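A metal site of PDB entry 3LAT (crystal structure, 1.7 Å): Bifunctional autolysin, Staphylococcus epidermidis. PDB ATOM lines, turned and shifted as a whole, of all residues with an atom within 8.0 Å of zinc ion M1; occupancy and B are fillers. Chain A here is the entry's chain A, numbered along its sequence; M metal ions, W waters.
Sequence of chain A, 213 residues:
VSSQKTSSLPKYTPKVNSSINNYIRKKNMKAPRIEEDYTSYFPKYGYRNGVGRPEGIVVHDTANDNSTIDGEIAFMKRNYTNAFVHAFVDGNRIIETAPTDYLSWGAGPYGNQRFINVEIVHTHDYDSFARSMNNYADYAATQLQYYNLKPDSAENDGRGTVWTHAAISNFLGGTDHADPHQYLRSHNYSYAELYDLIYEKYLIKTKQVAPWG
The backbone NH of Asp 61 lies close to the side-chain carboxylate of Asp 179. The backbone carbonyl oxygen (O) of Asp 179 lies within hydrogen-bond range of the backbone NH (N) of Ala 166, 3.1 Å away. N of His 165 lies within hydrogen-bond range of O of Val 59 (3.2 Å). NE2 of His 165 lies within hydrogen-bond range of OG1 of Thr 175 (2.7 Å). O of His 165 sits at hydrogen-bond distance from OG of Ser 169 (3.3 Å). The side-chain amide oxygen (OD1) of Asn 117 lies within hydrogen-bond range of a ring nitrogen (NE2) of His 60, 2.8 Å away. The backbone carbonyl oxygen (O) of Val 118 lies within hydrogen-bond range of the backbone NH (N) of His 60.
Within 4 Å of zinc ion M1: His 60, His 165 and Asp 179.
Zinc ion M1 is bound by OD2 of Asp 179 (2.0 Å), water W1 (2.0 Å), ND1 of His 165 (2.1 Å) and ND1 of His 60 (2.1 Å). Slightly farther from zinc ion M1 lies OD1 of Asp 179 (2.7 Å).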
ATOM      1  N   VAL A  58     -13.196 -10.082   9.267  1.00  0.00           N
ATOM      2  CA  VAL A  58     -12.407 -10.061  10.505  1.00  0.00           C
ATOM      3  C   VAL A  58     -13.303  -9.758  11.700  1.00  0.00           C
ATOM      4  O   VAL A  58     -14.173  -8.871  11.621  1.00  0.00           O
ATOM      5  CB  VAL A  58     -11.297  -8.994  10.490  1.00  0.00           C
ATOM      6  CG1 VAL A  58     -10.398  -9.120  11.744  1.00  0.00           C
ATOM      7  CG2 VAL A  58     -10.487  -9.082   9.224  1.00  0.00           C
ATOM      8  N   VAL A  59     -13.074 -10.471  12.794  1.00  0.00           N
ATOM      9  CA  VAL A  59     -13.762 -10.187  14.068  1.00  0.00           C
ATOM     10  C   VAL A  59     -12.879  -9.316  14.956  1.00  0.00           C
ATOM     11  O   VAL A  59     -11.795  -9.754  15.393  1.00  0.00           O
ATOM     12  CB  VAL A  59     -14.126 -11.485  14.858  1.00  0.00           C
ATOM     13  CG1 VAL A  59     -15.180 -11.170  15.923  1.00  0.00           C
ATOM     14  CG2 VAL A  59     -14.625 -12.596  13.919  1.00  0.00           C
ATOM     15  N   HIS A  60     -13.351  -8.089  15.199  1.00  0.00           N
ATOM     16  CA  HIS A  60     -12.683  -7.175  16.127  1.00  0.00           C
ATOM     17  C   HIS A  60     -13.601  -6.867  17.312  1.00  0.00           C
ATOM     18  O   HIS A  60     -14.827  -6.990  17.201  1.00  0.00           O
ATOM     19  CB  HIS A  60     -12.414  -5.814  15.485  1.00  0.00           C
ATOM     20  CG  HIS A  60     -11.501  -5.853  14.300  1.00  0.00           C
ATOM     21  ND1 HIS A  60     -10.128  -5.805  14.413  1.00  0.00           N
ATOM     22  CD2 HIS A  60     -11.775  -5.854  12.964  1.00  0.00           C
ATOM     23  CE1 HIS A  60      -9.592  -5.816  13.202  1.00  0.00           C
ATOM     24  NE2 HIS A  60     -10.569  -5.845  12.306  1.00  0.00           N
ATOM     25  N   ASP A  61     -13.011  -6.430  18.412  1.00  0.00           N
ATOM     26  CA  ASP A  61     -13.805  -5.690  19.412  1.00  0.00           C
ATOM     27  C   ASP A  61     -13.198  -4.302  19.565  1.00  0.00           C
ATOM     28  O   ASP A  61     -11.994  -4.099  19.340  1.00  0.00           O
ATOM     29  CB  ASP A  61     -13.939  -6.449  20.730  1.00  0.00           C
ATOM     30  CG  ASP A  61     -12.656  -6.441  21.572  1.00  0.00           C
ATOM     31  OD1 ASP A  61     -11.920  -7.450  21.560  1.00  0.00           O
ATOM     32  OD2 ASP A  61     -12.394  -5.418  22.252  1.00  0.00           O
ATOM     33  N   THR A  62     -14.034  -3.327  19.917  1.00  0.00           N
ATOM     34  CA  THR A  62     -13.598  -1.935  19.974  1.00  0.00           C
ATOM     35  C   THR A  62     -12.547  -1.724  21.073  1.00  0.00           C
ATOM     36  O   THR A  62     -12.547  -2.408  22.090  1.00  0.00           O
ATOM     37  CB  THR A  62     -14.783  -0.979  20.181  1.00  0.00           C
ATOM     38  OG1 THR A  62     -15.522  -1.402  21.340  1.00  0.00           O
ATOM     39  CG2 THR A  62     -15.695  -0.969  18.936  1.00  0.00           C
ATOM     40  N   ALA A  63     -11.665  -0.773  20.834  1.00  0.00           N
ATOM     41  CA  ALA A  63     -10.524  -0.547  21.709  1.00  0.00           C
ATOM     42  C   ALA A  63     -10.938  -0.116  23.112  1.00  0.00           C
ATOM     43  O   ALA A  63     -10.264  -0.408  24.070  1.00  0.00           O
ATOM     44  CB  ALA A  63      -9.623   0.486  21.103  1.00  0.00           C
ATOM     45  N   VAL A  85     -12.988   1.316   9.680  1.00  0.00           N
ATOM     46  CA  VAL A  85     -13.469  -0.052   9.476  1.00  0.00           C
ATOM     47  C   VAL A  85     -14.737  -0.068   8.637  1.00  0.00           C
ATOM     48  O   VAL A  85     -15.302   0.981   8.340  1.00  0.00           O
ATOM     49  CB  VAL A  85     -13.710  -0.804  10.827  1.00  0.00           C
ATOM     50  CG1 VAL A  85     -12.390  -0.919  11.627  1.00  0.00           C
ATOM     51  CG2 VAL A  85     -14.806  -0.108  11.665  1.00  0.00           C
ATOM     52  N   GLY A 106      -8.029  -1.459   9.282  1.00  0.00           N
ATOM     53  CA  GLY A 106      -8.301  -1.959  10.624  1.00  0.00           C
ATOM     54  C   GLY A 106      -7.532  -3.182  11.123  1.00  0.00           C
ATOM     55  O   GLY A 106      -7.707  -3.581  12.267  1.00  0.00           O
ATOM     56  N   ALA A 107      -6.683  -3.777  10.286  1.00  0.00           N
ATOM     57  CA  ALA A 107      -6.045  -5.059  10.662  1.00  0.00           C
ATOM     58  C   ALA A 107      -4.581  -5.173  10.217  1.00  0.00           C
ATOM     59  O   ALA A 107      -4.067  -6.278  10.056  1.00  0.00           O
ATOM     60  CB  ALA A 107      -6.876  -6.244  10.112  1.00  0.00           C
ATOM     61  N   ASN A 117     -13.425  -5.539   7.659  1.00  0.00           N
ATOM     62  CA  ASN A 117     -13.168  -5.281   9.075  1.00  0.00           C
ATOM     63  C   ASN A 117     -14.436  -4.887   9.808  1.00  0.00           C
ATOM     64  O   ASN A 117     -15.008  -3.827   9.514  1.00  0.00           O
ATOM     65  CB  ASN A 117     -12.124  -4.166   9.245  1.00  0.00           C
ATOM     66  CG  ASN A 117     -10.719  -4.634   8.924  1.00  0.00           C
ATOM     67  OD1 ASN A 117     -10.188  -5.564   9.554  1.00  0.00           O
ATOM     68  ND2 ASN A 117     -10.105  -4.011   7.912  1.00  0.00           N
ATOM     69  N   VAL A 118     -14.853  -5.712  10.767  1.00  0.00           N
ATOM     70  CA  VAL A 118     -16.083  -5.456  11.525  1.00  0.00           C
ATOM     71  C   VAL A 118     -15.811  -5.401  13.023  1.00  0.00           C
ATOM     72  O   VAL A 118     -15.114  -6.276  13.572  1.00  0.00           O
ATOM     73  CB  VAL A 118     -17.160  -6.521  11.243  1.00  0.00           C
ATOM     74  CG1 VAL A 118     -18.489  -6.171  11.985  1.00  0.00           C
ATOM     75  CG2 VAL A 118     -17.391  -6.656   9.725  1.00  0.00           C
ATOM     76  N   GLU A 119     -16.365  -4.378  13.664  1.00  0.00           N
ATOM     77  CA  GLU A 119     -16.130  -4.099  15.079  1.00  0.00           C
ATOM     78  C   GLU A 119     -17.331  -4.457  15.945  1.00  0.00           C
ATOM     79  O   GLU A 119     -18.461  -4.043  15.646  1.00  0.00           O
ATOM     80  CB  GLU A 119     -15.884  -2.607  15.261  1.00  0.00           C
ATOM     81  CG  GLU A 119     -14.525  -2.131  14.800  1.00  0.00           C
ATOM     82  CD  GLU A 119     -13.404  -2.534  15.749  1.00  0.00           C
ATOM     83  OE1 GLU A 119     -12.223  -2.332  15.363  1.00  0.00           O
ATOM     84  OE2 GLU A 119     -13.692  -3.044  16.851  1.00  0.00           O
ATOM     85  N   THR A 164     -10.343 -14.029  13.250  1.00  0.00           N
ATOM     86  CA  THR A 164     -10.171 -13.090  14.357  1.00  0.00           C
ATOM     87  C   THR A 164      -8.966 -12.198  14.048  1.00  0.00           C
ATOM     88  O   THR A 164      -8.075 -12.579  13.280  1.00  0.00           O
ATOM     89  CB  THR A 164      -9.904 -13.804  15.687  1.00  0.00           C
ATOM     90  OG1 THR A 164      -8.721 -14.622  15.584  1.00  0.00           O
ATOM     91  CG2 THR A 164     -11.096 -14.658  16.088  1.00  0.00           C
ATOM     92  N   HIS A 165      -8.915 -11.022  14.663  1.00  0.00           N
ATOM     93  CA  HIS A 165      -7.709 -10.222  14.581  1.00  0.00           C
ATOM     94  C   HIS A 165      -6.506 -11.048  15.106  1.00  0.00           C
ATOM     95  O   HIS A 165      -5.409 -10.994  14.526  1.00  0.00           O
ATOM     96  CB  HIS A 165      -7.863  -8.917  15.369  1.00  0.00           C
ATOM     97  CG  HIS A 165      -6.883  -7.863  14.992  1.00  0.00           C
ATOM     98  ND1 HIS A 165      -7.158  -6.525  15.126  1.00  0.00           N
ATOM     99  CD2 HIS A 165      -5.620  -7.946  14.470  1.00  0.00           C
ATOM    100  CE1 HIS A 165      -6.113  -5.813  14.718  1.00  0.00           C
ATOM    101  NE2 HIS A 165      -5.172  -6.649  14.314  1.00  0.00           N
ATOM    102  N   ALA A 166      -6.718 -11.834  16.151  1.00  0.00           N
ATOM    103  CA  ALA A 166      -5.674 -12.730  16.663  1.00  0.00           C
ATOM    104  C   ALA A 166      -5.089 -13.646  15.584  1.00  0.00           C
ATOM    105  O   ALA A 166      -3.866 -13.808  15.495  1.00  0.00           O
ATOM    106  CB  ALA A 166      -6.222 -13.564  17.813  1.00  0.00           C
ATOM    107  N   ILE A 168      -5.140 -13.131  12.305  1.00  0.00           N
ATOM    108  CA  ILE A 168      -4.349 -12.286  11.383  1.00  0.00           C
ATOM    109  C   ILE A 168      -2.955 -12.067  11.976  1.00  0.00           C
ATOM    110  O   ILE A 168      -1.941 -12.259  11.310  1.00  0.00           O
ATOM    111  CB  ILE A 168      -5.040 -10.941  11.096  1.00  0.00           C
ATOM    112  CG1 ILE A 168      -6.403 -11.203  10.414  1.00  0.00           C
ATOM    113  CG2 ILE A 168      -4.153 -10.040  10.215  1.00  0.00           C
ATOM    114  CD1 ILE A 168      -7.186  -9.954  10.117  1.00  0.00           C
ATOM    115  N   SER A 169      -2.913 -11.685  13.256  1.00  0.00           N
ATOM    116  CA  SER A 169      -1.627 -11.445  13.922  1.00  0.00           C
ATOM    117  C   SER A 169      -0.719 -12.684  13.867  1.00  0.00           C
ATOM    118  O   SER A 169       0.484 -12.590  13.586  1.00  0.00           O
ATOM    119  CB  SER A 169      -1.869 -11.023  15.378  1.00  0.00           C
ATOM    120  OG  SER A 169      -2.517  -9.755  15.404  1.00  0.00           O
ATOM    121  N   THR A 175       0.526  -6.907  12.299  1.00  0.00           N
ATOM    122  CA  THR A 175      -0.308  -6.479  13.445  1.00  0.00           C
ATOM    123  C   THR A 175      -0.135  -7.515  14.552  1.00  0.00           C
ATOM    124  O   THR A 175       0.268  -8.661  14.283  1.00  0.00           O
ATOM    125  CB  THR A 175      -1.823  -6.358  13.050  1.00  0.00           C
ATOM    126  OG1 THR A 175      -2.586  -5.844  14.156  1.00  0.00           O
ATOM    127  CG2 THR A 175      -2.406  -7.724  12.599  1.00  0.00           C
ATOM    128  N   ASP A 176      -0.434  -7.120  15.789  1.00  0.00           N
ATOM    129  CA  ASP A 176      -0.290  -8.032  16.914  1.00  0.00           C
ATOM    130  C   ASP A 176      -1.509  -8.119  17.840  1.00  0.00           C
ATOM    131  O   ASP A 176      -1.458  -8.827  18.844  1.00  0.00           O
ATOM    132  CB  ASP A 176       0.970  -7.700  17.734  1.00  0.00           C
ATOM    133  CG  ASP A 176       0.937  -6.312  18.355  1.00  0.00           C
ATOM    134  OD1 ASP A 176      -0.052  -5.969  19.045  1.00  0.00           O
ATOM    135  OD2 ASP A 176       1.904  -5.567  18.153  1.00  0.00           O
ATOM    136  N   HIS A 177      -2.588  -7.429  17.493  1.00  0.00           N
ATOM    137  CA  HIS A 177      -3.771  -7.417  18.364  1.00  0.00           C
ATOM    138  C   HIS A 177      -4.354  -8.821  18.439  1.00  0.00           C
ATOM    139  O   HIS A 177      -4.317  -9.586  17.457  1.00  0.00           O
ATOM    140  CB  HIS A 177      -4.830  -6.425  17.852  1.00  0.00           C
ATOM    141  CG  HIS A 177      -4.348  -5.005  17.754  1.00  0.00           C
ATOM    142  ND1 HIS A 177      -5.194  -3.927  17.852  1.00  0.00           N
ATOM    143  CD2 HIS A 177      -3.109  -4.490  17.573  1.00  0.00           C
ATOM    144  CE1 HIS A 177      -4.500  -2.808  17.717  1.00  0.00           C
ATOM    145  NE2 HIS A 177      -3.232  -3.128  17.548  1.00  0.00           N
ATOM    146  N   ALA A 178      -4.894  -9.171  19.610  1.00  0.00           N
ATOM    147  CA  ALA A 178      -5.400 -10.523  19.855  1.00  0.00           C
ATOM    148  C   ALA A 178      -6.921 -10.547  20.073  1.00  0.00           C
ATOM    149  O   ALA A 178      -7.499 -11.558  20.539  1.00  0.00           O
ATOM    150  CB  ALA A 178      -4.659 -11.153  21.039  1.00  0.00           C
ATOM    151  N   ASP A 179      -7.588  -9.456  19.711  1.00  0.00           N
ATOM    152  CA  ASP A 179      -9.043  -9.414  19.812  1.00  0.00           C
ATOM    153  C   ASP A 179      -9.668 -10.437  18.845  1.00  0.00           C
ATOM    154  O   ASP A 179      -9.045 -10.773  17.833  1.00  0.00           O
ATOM    155  CB  ASP A 179      -9.597  -7.995  19.574  1.00  0.00           C
ATOM    156  CG  ASP A 179      -9.072  -7.340  18.305  1.00  0.00           C
ATOM    157  OD1 ASP A 179      -7.834  -7.336  18.090  1.00  0.00           O
ATOM    158  OD2 ASP A 179      -9.905  -6.782  17.528  1.00  0.00           O
ATOM    159  N   PRO A 180     -10.879 -10.930  19.155  1.00  0.00           N
ATOM    160  CA  PRO A 180     -11.752 -10.567  20.281  1.00  0.00           C
ATOM    161  C   PRO A 180     -11.695 -11.541  21.483  1.00  0.00           C
ATOM    162  O   PRO A 180     -12.583 -11.500  22.317  1.00  0.00           O
ATOM    163  CB  PRO A 180     -13.140 -10.665  19.640  1.00  0.00           C
ATOM    164  CG  PRO A 180     -13.003 -11.940  18.794  1.00  0.00           C
ATOM    165  CD  PRO A 180     -11.565 -11.899  18.256  1.00  0.00           C
HETATM  166 ZN    ZN M   1      -8.877  -5.839  16.078  1.00  0.00          ZN
HETATM  167 ZN    ZN M   2      -7.248  -3.773  18.369  1.00  0.00          ZN
HETATM  168  O   HOH W   1      -8.363  -4.041  16.842  1.00  0.00           O
